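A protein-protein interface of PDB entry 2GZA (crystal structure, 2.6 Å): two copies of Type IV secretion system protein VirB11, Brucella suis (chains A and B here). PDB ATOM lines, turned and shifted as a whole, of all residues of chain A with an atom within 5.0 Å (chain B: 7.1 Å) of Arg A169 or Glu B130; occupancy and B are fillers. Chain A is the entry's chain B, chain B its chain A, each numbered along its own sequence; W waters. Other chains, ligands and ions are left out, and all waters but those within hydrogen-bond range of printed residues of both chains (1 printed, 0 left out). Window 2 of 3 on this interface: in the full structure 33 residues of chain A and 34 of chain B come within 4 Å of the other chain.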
ATOM      1  N   MET A 165      22.415  -4.892 -13.969  1.00  0.00           N
ATOM      2  CA  MET A 165      21.857  -5.878 -14.883  1.00  0.00           C
ATOM      3  C   MET A 165      21.799  -5.347 -16.316  1.00  0.00           C
ATOM      4  O   MET A 165      22.273  -6.010 -17.232  1.00  0.00           O
ATOM      5  CB  MET A 165      20.482  -6.372 -14.435  1.00  0.00           C
ATOM      6  CG  MET A 165      20.003  -7.594 -15.241  1.00  0.00           C
ATOM      7  SD  MET A 165      18.264  -8.023 -15.036  1.00  0.00           S
ATOM      8  CE  MET A 165      17.472  -6.697 -15.936  1.00  0.00           C
ATOM      9  N   SER A 166      21.233  -4.154 -16.499  1.00  0.00           N
ATOM     10  CA  SER A 166      21.154  -3.531 -17.817  1.00  0.00           C
ATOM     11  C   SER A 166      22.539  -3.236 -18.352  1.00  0.00           C
ATOM     12  O   SER A 166      22.796  -3.399 -19.542  1.00  0.00           O
ATOM     13  CB  SER A 166      20.338  -2.247 -17.776  1.00  0.00           C
ATOM     14  OG  SER A 166      18.977  -2.512 -17.506  1.00  0.00           O
ATOM     15  N   PHE A 167      23.433  -2.811 -17.464  1.00  0.00           N
ATOM     16  CA  PHE A 167      24.822  -2.548 -17.818  1.00  0.00           C
ATOM     17  C   PHE A 167      25.476  -3.758 -18.464  1.00  0.00           C
ATOM     18  O   PHE A 167      26.113  -3.646 -19.507  1.00  0.00           O
ATOM     19  CB  PHE A 167      25.632  -2.109 -16.590  1.00  0.00           C
ATOM     20  CG  PHE A 167      27.095  -1.902 -16.879  1.00  0.00           C
ATOM     21  CD1 PHE A 167      27.561  -0.672 -17.331  1.00  0.00           C
ATOM     22  CD2 PHE A 167      28.000  -2.941 -16.730  1.00  0.00           C
ATOM     23  CE1 PHE A 167      28.916  -0.475 -17.619  1.00  0.00           C
ATOM     24  CE2 PHE A 167      29.347  -2.756 -17.019  1.00  0.00           C
ATOM     25  CZ  PHE A 167      29.806  -1.520 -17.468  1.00  0.00           C
ATOM     26  N   LEU A 168      25.321  -4.913 -17.828  1.00  0.00           N
ATOM     27  CA  LEU A 168      25.937  -6.140 -18.311  1.00  0.00           C
ATOM     28  C   LEU A 168      25.320  -6.616 -19.615  1.00  0.00           C
ATOM     29  O   LEU A 168      26.044  -7.049 -20.511  1.00  0.00           O
ATOM     30  CB  LEU A 168      25.877  -7.237 -17.249  1.00  0.00           C
ATOM     31  CG  LEU A 168      26.760  -7.037 -16.021  1.00  0.00           C
ATOM     32  CD1 LEU A 168      26.525  -8.171 -15.028  1.00  0.00           C
ATOM     33  CD2 LEU A 168      28.234  -6.929 -16.395  1.00  0.00           C
ATOM     34  N   ARG A 169      23.994  -6.530 -19.716  1.00  0.00           N
ATOM     35  CA  ARG A 169      23.295  -6.838 -20.959  1.00  0.00           C
ATOM     36  C   ARG A 169      23.763  -5.935 -22.097  1.00  0.00           C
ATOM     37  O   ARG A 169      24.077  -6.425 -23.182  1.00  0.00           O
ATOM     38  CB  ARG A 169      21.773  -6.753 -20.794  1.00  0.00           C
ATOM     39  CG  ARG A 169      21.029  -6.829 -22.118  1.00  0.00           C
ATOM     40  CD  ARG A 169      19.530  -6.832 -21.950  1.00  0.00           C
ATOM     41  NE  ARG A 169      19.044  -8.115 -21.448  1.00  0.00           N
ATOM     42  CZ  ARG A 169      18.353  -8.279 -20.323  1.00  0.00           C
ATOM     43  NH1 ARG A 169      18.033  -7.245 -19.556  1.00  0.00           N
ATOM     44  NH2 ARG A 169      17.971  -9.493 -19.969  1.00  0.00           N
ATOM     45  N   ARG A 170      23.819  -4.631 -21.844  1.00  0.00           N
ATOM     46  CA  ARG A 170      24.279  -3.690 -22.859  1.00  0.00           C
ATOM     47  C   ARG A 170      25.733  -3.925 -23.250  1.00  0.00           C
ATOM     48  O   ARG A 170      26.069  -3.874 -24.427  1.00  0.00           O
ATOM     49  CB  ARG A 170      24.049  -2.238 -22.442  1.00  0.00           C
ATOM     50  CG  ARG A 170      22.600  -1.779 -22.562  1.00  0.00           C
ATOM     51  CD  ARG A 170      22.066  -1.879 -23.992  1.00  0.00           C
ATOM     52  NE  ARG A 170      22.533  -0.789 -24.849  1.00  0.00           N
ATOM     53  CZ  ARG A 170      22.715  -0.885 -26.163  1.00  0.00           C
ATOM     54  NH1 ARG A 170      22.484  -2.023 -26.795  1.00  0.00           N
ATOM     55  NH2 ARG A 170      23.136   0.167 -26.845  1.00  0.00           N
ATOM     56  N   ALA A 171      26.581  -4.211 -22.268  1.00  0.00           N
ATOM     57  CA  ALA A 171      28.003  -4.442 -22.523  1.00  0.00           C
ATOM     58  C   ALA A 171      28.219  -5.571 -23.509  1.00  0.00           C
ATOM     59  O   ALA A 171      29.054  -5.452 -24.412  1.00  0.00           O
ATOM     60  CB  ALA A 171      28.759  -4.708 -21.231  1.00  0.00           C
ATOM     61  N   VAL A 172      27.453  -6.649 -23.341  1.00  0.00           N
ATOM     62  CA  VAL A 172      27.526  -7.807 -24.225  1.00  0.00           C
ATOM     63  C   VAL A 172      27.013  -7.454 -25.614  1.00  0.00           C
ATOM     64  O   VAL A 172      27.581  -7.871 -26.629  1.00  0.00           O
ATOM     65  CB  VAL A 172      26.717  -9.007 -23.669  1.00  0.00           C
ATOM     66  CG1 VAL A 172      26.742 -10.158 -24.653  1.00  0.00           C
ATOM     67  CG2 VAL A 172      27.259  -9.452 -22.315  1.00  0.00           C
ATOM     68  N   GLN A 173      25.934  -6.681 -25.650  1.00  0.00           N
ATOM     69  CA  GLN A 173      25.333  -6.256 -26.896  1.00  0.00           C
ATOM     70  C   GLN A 173      26.255  -5.302 -27.645  1.00  0.00           C
ATOM     71  O   GLN A 173      26.356  -5.359 -28.868  1.00  0.00           O
ATOM     72  CB  GLN A 173      23.996  -5.590 -26.622  1.00  0.00           C
ATOM     73  CG  GLN A 173      22.867  -6.562 -26.349  1.00  0.00           C
ATOM     74  CD  GLN A 173      21.607  -5.872 -25.896  1.00  0.00           C
ATOM     75  OE1 GLN A 173      20.565  -6.495 -25.748  1.00  0.00           O
ATOM     76  NE2 GLN A 173      21.697  -4.578 -25.668  1.00  0.00           N
ATOM     77  N   GLU A 198      23.090 -13.326 -23.736  1.00  0.00           N
ATOM     78  CA  GLU A 198      22.795 -11.977 -24.216  1.00  0.00           C
ATOM     79  C   GLU A 198      23.422 -11.691 -25.591  1.00  0.00           C
ATOM     80  O   GLU A 198      23.150 -10.661 -26.205  1.00  0.00           O
ATOM     81  CB  GLU A 198      23.235 -10.923 -23.194  1.00  0.00           C
ATOM     82  CG  GLU A 198      22.604 -11.060 -21.787  1.00  0.00           C
ATOM     83  CD  GLU A 198      21.078 -11.055 -21.778  1.00  0.00           C
ATOM     84  OE1 GLU A 198      20.494 -11.850 -21.021  1.00  0.00           O
ATOM     85  OE2 GLU A 198      20.452 -10.266 -22.511  1.00  0.00           O
ATOM     86  N   ARG B 127      21.233 -19.890 -15.290  1.00  0.00           N
ATOM     87  CA  ARG B 127      20.380 -18.781 -14.893  1.00  0.00           C
ATOM     88  C   ARG B 127      20.480 -17.715 -15.966  1.00  0.00           C
ATOM     89  O   ARG B 127      21.543 -17.532 -16.556  1.00  0.00           O
ATOM     90  CB  ARG B 127      20.854 -18.151 -13.580  1.00  0.00           C
ATOM     91  CG  ARG B 127      21.157 -19.086 -12.420  1.00  0.00           C
ATOM     92  CD  ARG B 127      21.119 -18.312 -11.100  1.00  0.00           C
ATOM     93  NE  ARG B 127      22.011 -18.861 -10.080  1.00  0.00           N
ATOM     94  CZ  ARG B 127      21.690 -19.854  -9.256  1.00  0.00           C
ATOM     95  NH1 ARG B 127      20.499 -20.432  -9.326  1.00  0.00           N
ATOM     96  NH2 ARG B 127      22.565 -20.283  -8.361  1.00  0.00           N
ATOM     97  N   THR B 128      19.381 -17.011 -16.215  1.00  0.00           N
ATOM     98  CA  THR B 128      19.414 -15.800 -17.026  1.00  0.00           C
ATOM     99  C   THR B 128      19.854 -14.640 -16.140  1.00  0.00           C
ATOM    100  O   THR B 128      19.951 -14.791 -14.919  1.00  0.00           O
ATOM    101  CB  THR B 128      18.030 -15.460 -17.616  1.00  0.00           C
ATOM    102  OG1 THR B 128      17.066 -15.358 -16.553  1.00  0.00           O
ATOM    103  CG2 THR B 128      17.584 -16.513 -18.620  1.00  0.00           C
ATOM    104  N   LEU B 129      20.113 -13.480 -16.743  1.00  0.00           N
ATOM    105  CA  LEU B 129      20.362 -12.277 -15.958  1.00  0.00           C
ATOM    106  C   LEU B 129      19.121 -11.892 -15.157  1.00  0.00           C
ATOM    107  O   LEU B 129      19.242 -11.364 -14.055  1.00  0.00           O
ATOM    108  CB  LEU B 129      20.804 -11.100 -16.827  1.00  0.00           C
ATOM    109  CG  LEU B 129      22.213 -10.998 -17.421  1.00  0.00           C
ATOM    110  CD1 LEU B 129      22.298  -9.738 -18.271  1.00  0.00           C
ATOM    111  CD2 LEU B 129      23.289 -10.988 -16.353  1.00  0.00           C
ATOM    112  N   GLU B 130      17.936 -12.146 -15.710  1.00  0.00           N
ATOM    113  CA  GLU B 130      16.689 -11.953 -14.964  1.00  0.00           C
ATOM    114  C   GLU B 130      16.573 -12.844 -13.718  1.00  0.00           C
ATOM    115  O   GLU B 130      16.156 -12.372 -12.668  1.00  0.00           O
ATOM    116  CB  GLU B 130      15.462 -12.098 -15.864  1.00  0.00           C
ATOM    117  CG  GLU B 130      15.039 -10.800 -16.518  1.00  0.00           C
ATOM    118  CD  GLU B 130      15.820 -10.484 -17.780  1.00  0.00           C
ATOM    119  OE1 GLU B 130      16.622 -11.329 -18.217  1.00  0.00           O
ATOM    120  OE2 GLU B 130      15.625  -9.390 -18.349  1.00  0.00           O
ATOM    121  N   ASP B 131      16.948 -14.117 -13.829  1.00  0.00           N
ATOM    122  CA  ASP B 131      16.936 -15.026 -12.671  1.00  0.00           C
ATOM    123  C   ASP B 131      17.858 -14.506 -11.583  1.00  0.00           C
ATOM    124  O   ASP B 131      17.495 -14.509 -10.401  1.00  0.00           O
ATOM    125  CB  ASP B 131      17.343 -16.457 -13.045  1.00  0.00           C
ATOM    126  CG  ASP B 131      16.490 -17.047 -14.149  1.00  0.00           C
ATOM    127  OD1 ASP B 131      15.240 -16.878 -14.140  1.00  0.00           O
ATOM    128  OD2 ASP B 131      17.087 -17.691 -15.034  1.00  0.00           O
ATOM    129  N   TYR B 132      19.052 -14.067 -11.993  1.00  0.00           N
ATOM    130  CA  TYR B 132      20.031 -13.471 -11.087  1.00  0.00           C
ATOM    131  C   TYR B 132      19.456 -12.274 -10.345  1.00  0.00           C
ATOM    132  O   TYR B 132      19.651 -12.142  -9.145  1.00  0.00           O
ATOM    133  CB  TYR B 132      21.282 -13.024 -11.840  1.00  0.00           C
ATOM    134  CG  TYR B 132      22.386 -14.046 -11.947  1.00  0.00           C
ATOM    135  CD1 TYR B 132      22.861 -14.454 -13.188  1.00  0.00           C
ATOM    136  CD2 TYR B 132      22.977 -14.595 -10.805  1.00  0.00           C
ATOM    137  CE1 TYR B 132      23.893 -15.382 -13.293  1.00  0.00           C
ATOM    138  CE2 TYR B 132      24.009 -15.523 -10.901  1.00  0.00           C
ATOM    139  CZ  TYR B 132      24.456 -15.911 -12.151  1.00  0.00           C
ATOM    140  OH  TYR B 132      25.466 -16.827 -12.267  1.00  0.00           O
ATOM    141  N   ALA B 133      18.751 -11.410 -11.069  1.00  0.00           N
ATOM    142  CA  ALA B 133      18.140 -10.218 -10.496  1.00  0.00           C
ATOM    143  C   ALA B 133      17.213 -10.553  -9.330  1.00  0.00           C
ATOM    144  O   ALA B 133      17.316  -9.943  -8.265  1.00  0.00           O
ATOM    145  CB  ALA B 133      17.395  -9.434 -11.558  1.00  0.00           C
ATOM    146  N   GLN B 134      16.330 -11.532  -9.532  1.00  0.00           N
ATOM    147  CA  GLN B 134      15.388 -11.976  -8.502  1.00  0.00           C
ATOM    148  C   GLN B 134      16.071 -12.650  -7.318  1.00  0.00           C
ATOM    149  O   GLN B 134      15.507 -12.708  -6.224  1.00  0.00           O
ATOM    150  CB  GLN B 134      14.330 -12.911  -9.089  1.00  0.00           C
ATOM    151  CG  GLN B 134      13.423 -12.267 -10.126  1.00  0.00           C
ATOM    152  CD  GLN B 134      12.746 -11.002  -9.625  1.00  0.00           C
ATOM    153  OE1 GLN B 134      12.110 -10.996  -8.564  1.00  0.00           O
ATOM    154  NE2 GLN B 134      12.884  -9.922 -10.388  1.00  0.00           N
ATOM    155  N   GLN B 135      17.274 -13.165  -7.538  1.00  0.00           N
ATOM    156  CA  GLN B 135      18.070 -13.740  -6.454  1.00  0.00           C
ATOM    157  C   GLN B 135      18.780 -12.659  -5.638  1.00  0.00           C
ATOM    158  O   GLN B 135      19.490 -12.972  -4.692  1.00  0.00           O
ATOM    159  CB  GLN B 135      19.109 -14.742  -6.995  1.00  0.00           C
ATOM    160  CG  GLN B 135      18.549 -16.096  -7.423  1.00  0.00           C
ATOM    161  CD  GLN B 135      17.709 -16.755  -6.342  1.00  0.00           C
ATOM    162  OE1 GLN B 135      16.562 -17.133  -6.581  1.00  0.00           O
ATOM    163  NE2 GLN B 135      18.275 -16.895  -5.141  1.00  0.00           N
ATOM    164  N   PHE B 138      22.278  -8.303  -7.818  1.00  0.00           N
ATOM    165  CA  PHE B 138      22.776  -6.967  -8.129  1.00  0.00           C
ATOM    166  C   PHE B 138      22.536  -5.958  -7.005  1.00  0.00           C
ATOM    167  O   PHE B 138      22.705  -4.759  -7.202  1.00  0.00           O
ATOM    168  CB  PHE B 138      22.157  -6.469  -9.429  1.00  0.00           C
ATOM    169  CG  PHE B 138      22.336  -7.403 -10.570  1.00  0.00           C
ATOM    170  CD1 PHE B 138      21.268  -8.159 -11.027  1.00  0.00           C
ATOM    171  CD2 PHE B 138      23.576  -7.539 -11.186  1.00  0.00           C
ATOM    172  CE1 PHE B 138      21.423  -9.031 -12.088  1.00  0.00           C
ATOM    173  CE2 PHE B 138      23.746  -8.410 -12.245  1.00  0.00           C
ATOM    174  CZ  PHE B 138      22.667  -9.156 -12.697  1.00  0.00           C
HETATM  175  O   HOH W   1      20.930 -14.030 -19.308  1.00  0.00           O
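The side-chain carboxylate (OE2) of Glu B130 is in salt-bridge range of the guanidinium group (NH2) of Arg A169 (2.9 Å). SD of Met A165 sits close to O of Leu B129 (3.6 Å).
Of the printed residues of chain B, Arg A169 touches Leu B129 and Glu B130. Of the printed residues of chain A, Glu B130 touches Arg A169 (2.9 Å). Of the printed residues of chain A, Phe B138 touches Met A165 and Leu A168. Of the printed residues of chain A, Leu B129 touches Met A165 (3.6 Å), Arg A169 (3.9 Å) and Glu A198 (3.8 Å). Of the printed residues of chain B, Met A165 touches Leu B129, Ala B133 and Phe B138. Of the printed residues of chain B, Glu A198 touches Leu B129 (3.8 Å). Of the printed residues of chain A, Ala B133 touches Met A165. The nearest residue of chain B that does not touch Arg A169 is Thr B128 (6.4 Å). The nearest residue of chain A that does not touch Glu B130 is Met A165 (4.1 Å).
The guanidinium group of Arg A169 is in salt-bridge range of the side-chain carboxylate of Glu A198, 2.8 Å away. The side-chain hydroxyl (OG1) of Thr B128 lies close to the backbone NH (N) of Glu B130, 3.4 Å away.
No position is printed for both chains. Of the 7 pairs that touch across the chains among the printed residues, none has its exchanged pair printed and touching as well.
Water W1 lies within hydrogen-bond range of the backbone NH (N) of Leu B129 and the side-chain carboxylate (OE1) of Glu A198.
Printed residues of chain B that touch a printed residue of chain A: Leu B129, Glu B130, Ala B133 and Phe B138. Of the 10 printed residues of chain A, 4 touch a printed residue of chain B.
SD of Met A165 touches CB of Ala B133, 3.9 Å away. Met A165 touches Phe B138. Leu A168 touches Phe B138. Leu B129 touches Arg A169. Glu A198 touches Leu B129 (CG to CD1, 3.8 Å).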
